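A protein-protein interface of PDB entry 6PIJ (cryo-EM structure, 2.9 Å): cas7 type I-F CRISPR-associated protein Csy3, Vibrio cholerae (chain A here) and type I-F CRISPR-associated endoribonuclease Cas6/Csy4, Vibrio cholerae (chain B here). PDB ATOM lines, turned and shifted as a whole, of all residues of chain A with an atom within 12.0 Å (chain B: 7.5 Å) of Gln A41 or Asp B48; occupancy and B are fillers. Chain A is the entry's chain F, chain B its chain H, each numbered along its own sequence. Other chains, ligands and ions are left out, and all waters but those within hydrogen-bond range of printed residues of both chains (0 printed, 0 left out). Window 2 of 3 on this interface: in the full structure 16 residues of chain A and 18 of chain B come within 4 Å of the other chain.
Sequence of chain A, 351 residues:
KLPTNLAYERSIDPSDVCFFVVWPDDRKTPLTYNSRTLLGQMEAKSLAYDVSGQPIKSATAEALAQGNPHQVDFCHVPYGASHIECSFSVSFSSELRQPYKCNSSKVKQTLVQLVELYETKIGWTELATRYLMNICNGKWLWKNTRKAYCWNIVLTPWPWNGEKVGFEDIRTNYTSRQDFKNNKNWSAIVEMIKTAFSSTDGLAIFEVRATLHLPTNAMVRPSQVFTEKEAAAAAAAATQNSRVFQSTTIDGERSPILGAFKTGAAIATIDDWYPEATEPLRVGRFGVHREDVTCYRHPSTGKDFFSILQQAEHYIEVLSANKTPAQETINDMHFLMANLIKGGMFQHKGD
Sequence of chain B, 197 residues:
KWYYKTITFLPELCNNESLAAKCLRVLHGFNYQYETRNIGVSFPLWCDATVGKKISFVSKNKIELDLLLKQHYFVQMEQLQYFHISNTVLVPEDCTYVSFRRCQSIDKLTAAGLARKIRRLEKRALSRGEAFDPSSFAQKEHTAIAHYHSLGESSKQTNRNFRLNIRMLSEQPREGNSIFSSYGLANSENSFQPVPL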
ATOM      1  N   THR A  37      27.070 -17.366   1.490  1.00  0.00           N
ATOM      2  CA  THR A  37      26.640 -18.074   0.253  1.00  0.00           C
ATOM      3  C   THR A  37      27.257 -19.479   0.249  1.00  0.00           C
ATOM      4  O   THR A  37      28.485 -19.576   0.429  1.00  0.00           O
ATOM      5  CB  THR A  37      27.044 -17.295  -1.005  1.00  0.00           C
ATOM      6  OG1 THR A  37      26.600 -15.945  -0.861  1.00  0.00           O
ATOM      7  CG2 THR A  37      26.470 -17.885  -2.275  1.00  0.00           C
ATOM      8  N   LEU A  38      26.434 -20.517   0.056  1.00  0.00           N
ATOM      9  CA  LEU A  38      26.883 -21.934  -0.025  1.00  0.00           C
ATOM     10  C   LEU A  38      27.267 -22.250  -1.478  1.00  0.00           C
ATOM     11  O   LEU A  38      26.358 -22.533  -2.286  1.00  0.00           O
ATOM     12  CB  LEU A  38      25.773 -22.855   0.498  1.00  0.00           C
ATOM     13  CG  LEU A  38      25.351 -22.626   1.950  1.00  0.00           C
ATOM     14  CD1 LEU A  38      24.259 -23.605   2.357  1.00  0.00           C
ATOM     15  CD2 LEU A  38      26.540 -22.733   2.896  1.00  0.00           C
ATOM     16  N   LEU A  39      28.569 -22.187  -1.787  1.00  0.00           N
ATOM     17  CA  LEU A  39      29.154 -22.421  -3.138  1.00  0.00           C
ATOM     18  C   LEU A  39      28.982 -23.906  -3.498  1.00  0.00           C
ATOM     19  O   LEU A  39      29.969 -24.661  -3.417  1.00  0.00           O
ATOM     20  CB  LEU A  39      30.626 -21.978  -3.129  1.00  0.00           C
ATOM     21  CG  LEU A  39      31.263 -21.698  -4.494  1.00  0.00           C
ATOM     22  CD1 LEU A  39      32.405 -20.697  -4.361  1.00  0.00           C
ATOM     23  CD2 LEU A  39      31.757 -22.972  -5.168  1.00  0.00           C
ATOM     24  N   GLY A  40      27.762 -24.302  -3.883  1.00  0.00           N
ATOM     25  CA  GLY A  40      27.385 -25.696  -4.201  1.00  0.00           C
ATOM     26  C   GLY A  40      28.395 -26.355  -5.127  1.00  0.00           C
ATOM     27  O   GLY A  40      28.763 -25.720  -6.137  1.00  0.00           O
ATOM     28  N   GLN A  41      28.827 -27.581  -4.799  1.00  0.00           N
ATOM     29  CA  GLN A  41      29.959 -28.283  -5.468  1.00  0.00           C
ATOM     30  C   GLN A  41      29.595 -28.613  -6.924  1.00  0.00           C
ATOM     31  O   GLN A  41      28.405 -28.506  -7.289  1.00  0.00           O
ATOM     32  CB  GLN A  41      30.369 -29.541  -4.691  1.00  0.00           C
ATOM     33  CG  GLN A  41      29.438 -30.736  -4.869  1.00  0.00           C
ATOM     34  CD  GLN A  41      30.028 -32.003  -4.300  1.00  0.00           C
ATOM     35  OE1 GLN A  41      30.379 -32.929  -5.029  1.00  0.00           O
ATOM     36  NE2 GLN A  41      30.153 -32.049  -2.984  1.00  0.00           N
ATOM     37  N   MET A  42      30.596 -29.027  -7.704  1.00  0.00           N
ATOM     38  CA  MET A  42      30.485 -29.307  -9.162  1.00  0.00           C
ATOM     39  C   MET A  42      29.848 -30.686  -9.365  1.00  0.00           C
ATOM     40  O   MET A  42      29.413 -30.950 -10.503  1.00  0.00           O
ATOM     41  CB  MET A  42      31.864 -29.276  -9.833  1.00  0.00           C
ATOM     42  CG  MET A  42      32.521 -27.904  -9.830  1.00  0.00           C
ATOM     43  SD  MET A  42      32.846 -27.242  -8.173  1.00  0.00           S
ATOM     44  CE  MET A  42      34.135 -28.351  -7.605  1.00  0.00           C
ATOM     45  N   PRO A  69      23.759 -16.503  -5.704  1.00  0.00           N
ATOM     46  CA  PRO A  69      22.391 -16.819  -6.137  1.00  0.00           C
ATOM     47  C   PRO A  69      21.490 -17.104  -4.924  1.00  0.00           C
ATOM     48  O   PRO A  69      20.535 -16.368  -4.735  1.00  0.00           O
ATOM     49  CB  PRO A  69      22.507 -18.045  -7.064  1.00  0.00           C
ATOM     50  CG  PRO A  69      23.994 -18.288  -7.205  1.00  0.00           C
ATOM     51  CD  PRO A  69      24.624 -17.646  -5.988  1.00  0.00           C
ATOM     52  N   HIS A  70      21.816 -18.144  -4.145  1.00  0.00           N
ATOM     53  CA  HIS A  70      21.157 -18.494  -2.855  1.00  0.00           C
ATOM     54  C   HIS A  70      21.980 -17.885  -1.712  1.00  0.00           C
ATOM     55  O   HIS A  70      22.624 -18.643  -0.955  1.00  0.00           O
ATOM     56  CB  HIS A  70      20.951 -20.013  -2.739  1.00  0.00           C
ATOM     57  CG  HIS A  70      20.068 -20.413  -1.604  1.00  0.00           C
ATOM     58  ND1 HIS A  70      20.560 -20.680  -0.339  1.00  0.00           N
ATOM     59  CD2 HIS A  70      18.730 -20.587  -1.532  1.00  0.00           C
ATOM     60  CE1 HIS A  70      19.564 -21.003   0.460  1.00  0.00           C
ATOM     61  NE2 HIS A  70      18.430 -20.954  -0.248  1.00  0.00           N
ATOM     62  N   GLU B  17      19.677 -37.492   6.109  1.00  0.00           N
ATOM     63  CA  GLU B  17      20.525 -36.927   7.199  1.00  0.00           C
ATOM     64  C   GLU B  17      19.970 -37.357   8.566  1.00  0.00           C
ATOM     65  O   GLU B  17      20.792 -37.674   9.453  1.00  0.00           O
ATOM     66  CB  GLU B  17      20.615 -35.398   7.115  1.00  0.00           C
ATOM     67  CG  GLU B  17      21.513 -34.888   5.996  1.00  0.00           C
ATOM     68  CD  GLU B  17      20.901 -34.816   4.605  1.00  0.00           C
ATOM     69  OE1 GLU B  17      19.691 -35.089   4.464  1.00  0.00           O
ATOM     70  OE2 GLU B  17      21.644 -34.486   3.658  1.00  0.00           O
ATOM     71  N   LEU B  45      26.698 -43.124  -1.968  1.00  0.00           N
ATOM     72  CA  LEU B  45      25.830 -42.312  -2.867  1.00  0.00           C
ATOM     73  C   LEU B  45      25.791 -40.854  -2.378  1.00  0.00           C
ATOM     74  O   LEU B  45      24.707 -40.234  -2.436  1.00  0.00           O
ATOM     75  CB  LEU B  45      24.429 -42.936  -2.900  1.00  0.00           C
ATOM     76  CG  LEU B  45      24.223 -44.104  -3.861  1.00  0.00           C
ATOM     77  CD1 LEU B  45      25.038 -45.316  -3.443  1.00  0.00           C
ATOM     78  CD2 LEU B  45      22.746 -44.459  -3.948  1.00  0.00           C
ATOM     79  N   TRP B  46      26.930 -40.317  -1.923  1.00  0.00           N
ATOM     80  CA  TRP B  46      27.090 -38.888  -1.541  1.00  0.00           C
ATOM     81  C   TRP B  46      27.062 -38.040  -2.818  1.00  0.00           C
ATOM     82  O   TRP B  46      28.090 -38.001  -3.526  1.00  0.00           O
ATOM     83  CB  TRP B  46      28.379 -38.680  -0.729  1.00  0.00           C
ATOM     84  CG  TRP B  46      28.640 -37.271  -0.281  1.00  0.00           C
ATOM     85  CD1 TRP B  46      28.996 -36.205  -1.057  1.00  0.00           C
ATOM     86  CD2 TRP B  46      28.607 -36.782   1.072  1.00  0.00           C
ATOM     87  NE1 TRP B  46      29.165 -35.085  -0.288  1.00  0.00           N
ATOM     88  CE2 TRP B  46      28.936 -35.408   1.022  1.00  0.00           C
ATOM     89  CE3 TRP B  46      28.324 -37.363   2.315  1.00  0.00           C
ATOM     90  CZ2 TRP B  46      28.990 -34.615   2.167  1.00  0.00           C
ATOM     91  CZ3 TRP B  46      28.376 -36.578   3.446  1.00  0.00           C
ATOM     92  CH2 TRP B  46      28.706 -35.224   3.369  1.00  0.00           C
ATOM     93  N   CYS B  47      25.908 -37.436  -3.119  1.00  0.00           N
ATOM     94  CA  CYS B  47      25.724 -36.391  -4.164  1.00  0.00           C
ATOM     95  C   CYS B  47      25.726 -35.017  -3.481  1.00  0.00           C
ATOM     96  O   CYS B  47      25.897 -34.979  -2.245  1.00  0.00           O
ATOM     97  CB  CYS B  47      24.444 -36.636  -4.958  1.00  0.00           C
ATOM     98  SG  CYS B  47      22.989 -36.926  -3.920  1.00  0.00           S
ATOM     99  N   ASP B  48      25.579 -33.935  -4.253  1.00  0.00           N
ATOM    100  CA  ASP B  48      25.633 -32.530  -3.759  1.00  0.00           C
ATOM    101  C   ASP B  48      24.432 -32.230  -2.846  1.00  0.00           C
ATOM    102  O   ASP B  48      24.607 -31.450  -1.897  1.00  0.00           O
ATOM    103  CB  ASP B  48      25.718 -31.527  -4.915  1.00  0.00           C
ATOM    104  CG  ASP B  48      24.504 -31.504  -5.831  1.00  0.00           C
ATOM    105  OD1 ASP B  48      23.895 -32.576  -6.028  1.00  0.00           O
ATOM    106  OD2 ASP B  48      24.177 -30.414  -6.341  1.00  0.00           O
ATOM    107  N   ALA B  49      23.256 -32.803  -3.130  1.00  0.00           N
ATOM    108  CA  ALA B  49      22.017 -32.615  -2.338  1.00  0.00           C
ATOM    109  C   ALA B  49      21.353 -33.972  -2.087  1.00  0.00           C
ATOM    110  O   ALA B  49      21.220 -34.747  -3.054  1.00  0.00           O
ATOM    111  CB  ALA B  49      21.084 -31.672  -3.055  1.00  0.00           C
ATOM    112  N   THR B  50      20.953 -34.229  -0.836  1.00  0.00           N
ATOM    113  CA  THR B  50      20.329 -35.496  -0.366  1.00  0.00           C
ATOM    114  C   THR B  50      21.354 -36.628  -0.516  1.00  0.00           C
ATOM    115  O   THR B  50      21.273 -37.366  -1.522  1.00  0.00           O
ATOM    116  CB  THR B  50      19.002 -35.756  -1.099  1.00  0.00           C
ATOM    117  OG1 THR B  50      18.198 -34.581  -0.994  1.00  0.00           O
ATOM    118  CG2 THR B  50      18.234 -36.939  -0.552  1.00  0.00           C
ATOM    119  N   VAL B  51      22.301 -36.726   0.429  1.00  0.00           N
ATOM    120  CA  VAL B  51      23.233 -37.888   0.586  1.00  0.00           C
ATOM    121  C   VAL B  51      22.398 -39.170   0.466  1.00  0.00           C
ATOM    122  O   VAL B  51      21.327 -39.231   1.093  1.00  0.00           O
ATOM    123  CB  VAL B  51      24.033 -37.841   1.907  1.00  0.00           C
ATOM    124  CG1 VAL B  51      23.144 -37.761   3.143  1.00  0.00           C
ATOM    125  CG2 VAL B  51      24.994 -39.015   2.028  1.00  0.00           C
ATOM    126  N   ILE B 145      31.105 -20.634   1.170  1.00  0.00           N
ATOM    127  CA  ILE B 145      31.282 -21.914   1.924  1.00  0.00           C
ATOM    128  C   ILE B 145      30.824 -23.077   1.035  1.00  0.00           C
ATOM    129  O   ILE B 145      29.935 -22.859   0.197  1.00  0.00           O
ATOM    130  CB  ILE B 145      30.502 -21.869   3.257  1.00  0.00           C
ATOM    131  CG1 ILE B 145      30.744 -20.569   4.033  1.00  0.00           C
ATOM    132  CG2 ILE B 145      30.803 -23.092   4.110  1.00  0.00           C
ATOM    133  CD1 ILE B 145      32.188 -20.331   4.423  1.00  0.00           C
ATOM    134  N   ALA B 146      31.419 -24.263   1.209  1.00  0.00           N
ATOM    135  CA  ALA B 146      31.043 -25.524   0.522  1.00  0.00           C
ATOM    136  C   ALA B 146      31.754 -26.697   1.190  1.00  0.00           C
ATOM    137  O   ALA B 146      32.957 -26.597   1.413  1.00  0.00           O
ATOM    138  CB  ALA B 146      31.418 -25.451  -0.935  1.00  0.00           C
ATOM    139  N   HIS B 147      31.073 -27.819   1.475  1.00  0.00           N
ATOM    140  CA  HIS B 147      29.719 -28.153   1.053  1.00  0.00           C
ATOM    141  C   HIS B 147      28.953 -28.695   2.269  1.00  0.00           C
ATOM    142  O   HIS B 147      27.830 -28.219   2.528  1.00  0.00           O
ATOM    143  CB  HIS B 147      29.803 -29.133  -0.124  1.00  0.00           C
ATOM    144  CG  HIS B 147      28.501 -29.395  -0.798  1.00  0.00           C
ATOM    145  ND1 HIS B 147      27.736 -28.385  -1.346  1.00  0.00           N
ATOM    146  CD2 HIS B 147      27.842 -30.547  -1.035  1.00  0.00           C
ATOM    147  CE1 HIS B 147      26.652 -28.904  -1.882  1.00  0.00           C
ATOM    148  NE2 HIS B 147      26.698 -30.226  -1.707  1.00  0.00           N
ATOM    149  N   TYR B 148      29.527 -29.712   2.924  1.00  0.00           N
ATOM    150  CA  TYR B 148      29.541 -29.967   4.393  1.00  0.00           C
ATOM    151  C   TYR B 148      28.275 -30.666   4.920  1.00  0.00           C
ATOM    152  O   TYR B 148      28.333 -31.032   6.110  1.00  0.00           O
ATOM    153  CB  TYR B 148      29.907 -28.699   5.178  1.00  0.00           C
ATOM    154  CG  TYR B 148      28.836 -27.658   5.410  1.00  0.00           C
ATOM    155  CD1 TYR B 148      27.831 -27.843   6.350  1.00  0.00           C
ATOM    156  CD2 TYR B 148      28.871 -26.441   4.744  1.00  0.00           C
ATOM    157  CE1 TYR B 148      26.866 -26.876   6.584  1.00  0.00           C
ATOM    158  CE2 TYR B 148      27.913 -25.463   4.966  1.00  0.00           C
ATOM    159  CZ  TYR B 148      26.906 -25.680   5.890  1.00  0.00           C
ATOM    160  OH  TYR B 148      25.961 -24.723   6.116  1.00  0.00           O
ATOM    161  N   HIS B 149      27.219 -30.868   4.115  1.00  0.00           N
ATOM    162  CA  HIS B 149      26.013 -31.685   4.448  1.00  0.00           C
ATOM    163  C   HIS B 149      25.940 -31.984   5.955  1.00  0.00           C
ATOM    164  O   HIS B 149      26.363 -33.086   6.370  1.00  0.00           O
ATOM    165  CB  HIS B 149      26.013 -32.987   3.625  1.00  0.00           C
ATOM    166  CG  HIS B 149      25.225 -32.948   2.358  1.00  0.00           C
ATOM    167  ND1 HIS B 149      25.321 -33.952   1.414  1.00  0.00           N
ATOM    168  CD2 HIS B 149      24.331 -32.057   1.875  1.00  0.00           C
ATOM    169  CE1 HIS B 149      24.519 -33.681   0.406  1.00  0.00           C
ATOM    170  NE2 HIS B 149      23.900 -32.526   0.664  1.00  0.00           N
ATOM    171  N   ARG B 167      32.646 -33.332   4.979  1.00  0.00           N
ATOM    172  CA  ARG B 167      32.998 -33.076   3.552  1.00  0.00           C
ATOM    173  C   ARG B 167      33.578 -34.343   2.912  1.00  0.00           C
ATOM    174  O   ARG B 167      34.392 -35.014   3.576  1.00  0.00           O
ATOM    175  CB  ARG B 167      34.033 -31.953   3.444  1.00  0.00           C
ATOM    176  CG  ARG B 167      33.465 -30.549   3.584  1.00  0.00           C
ATOM    177  CD  ARG B 167      34.531 -29.527   3.241  1.00  0.00           C
ATOM    178  NE  ARG B 167      34.021 -28.164   3.200  1.00  0.00           N
ATOM    179  CZ  ARG B 167      33.836 -27.361   4.249  1.00  0.00           C
ATOM    180  NH1 ARG B 167      33.365 -26.140   4.049  1.00  0.00           N
ATOM    181  NH2 ARG B 167      34.109 -27.764   5.479  1.00  0.00           N
ATOM    182  N   MET B 168      33.197 -34.615   1.657  1.00  0.00           N
ATOM    183  CA  MET B 168      33.744 -35.707   0.804  1.00  0.00           C
ATOM    184  C   MET B 168      34.894 -35.155  -0.049  1.00  0.00           C
ATOM    185  O   MET B 168      34.764 -34.023  -0.556  1.00  0.00           O
ATOM    186  CB  MET B 168      32.658 -36.275  -0.119  1.00  0.00           C
ATOM    187  CG  MET B 168      33.136 -37.424  -0.999  1.00  0.00           C
ATOM    188  SD  MET B 168      31.822 -38.125  -2.027  1.00  0.00           S
ATOM    189  CE  MET B 168      31.572 -36.800  -3.209  1.00  0.00           C
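The backbone NH (N) of Leu A39 sits at hydrogen-bond distance from the backbone carbonyl oxygen (O) of Ile B145 (2.5 Å). N of Ile B145 lies within hydrogen-bond range of O of Thr A37 (2.9 Å).
A ring nitrogen (NE2) of His B147 lies within hydrogen-bond range of the backbone carbonyl oxygen (O) of Asp B48, at 2.4 Å. O of Asp B48 lies within hydrogen-bond range of NE2 of His B149, at 2.9 Å. NE of Arg B167 is in hydrogen-bond range of O of Ala B146.
Leu A38 touches Ile B145 (CA to O, 3.2 Å). Leu A38 touches Tyr B148. Leu A39 touches Ala B146. Gly A40 touches His B147 (CA to ND1, 3.9 Å). Asp B48 touches Gln A41 (CB to CG, 3.8 Å). Gln A41 touches His B147 (NE2 to CD2, 3.4 Å).
Of the printed residues of chain B, Leu A38 touches Ile B145 (3.2 Å) and Tyr B148 (3.7 Å). Of the printed residues of chain B, Leu A39 touches Ile B145 and Ala B146. Printed residues of chain B within 4 Å of Gly A40: His B147 (3.9 Å). Gln A41 touches two residues of chain B. Cys B47 touches none of the printed residues of chain A. Of chain A, only Gln A41 (3.8 Å) comes within 4 Å of Asp B48. No residue of chain A comes within 4 Å of Ala B49. Ala B146 touches just one residue of chain A: Leu A39 (3.0 Å). His B147 touches just these residues of chain A: Gly A40 and Gln A41. Printed residues of chain A within 4 Å of Tyr B148: Leu A38. The nearest residue of chain B that does not touch Gln A41 is Trp B46 (4.2 Å). The nearest residue of chain A that does not touch Asp B48 is Gly A40 (5.8 Å).
Of the 15 printed residues of chain B, 5 touch a printed residue of chain A. Printed residues of chain B that touch a printed residue of chain A: Asp B48, Ile B145, Ala B146, His B147 and Tyr B148. Hydrophobic or aromatic side chains of chain B within 4 Å of the printed part of chain A: Ala B146, His B147 and Tyr B148. Along chain B the printed residues that touch a printed residue of chain A span positions 48 to 148. Of the 8 printed residues of chain A, 5 touch a printed residue of chain B. Hydrophobic or aromatic side chains of chain A that line the printed part of chain B: Leu A38 and Leu A39. Among the printed residues, 8 pairs touch across the chains.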
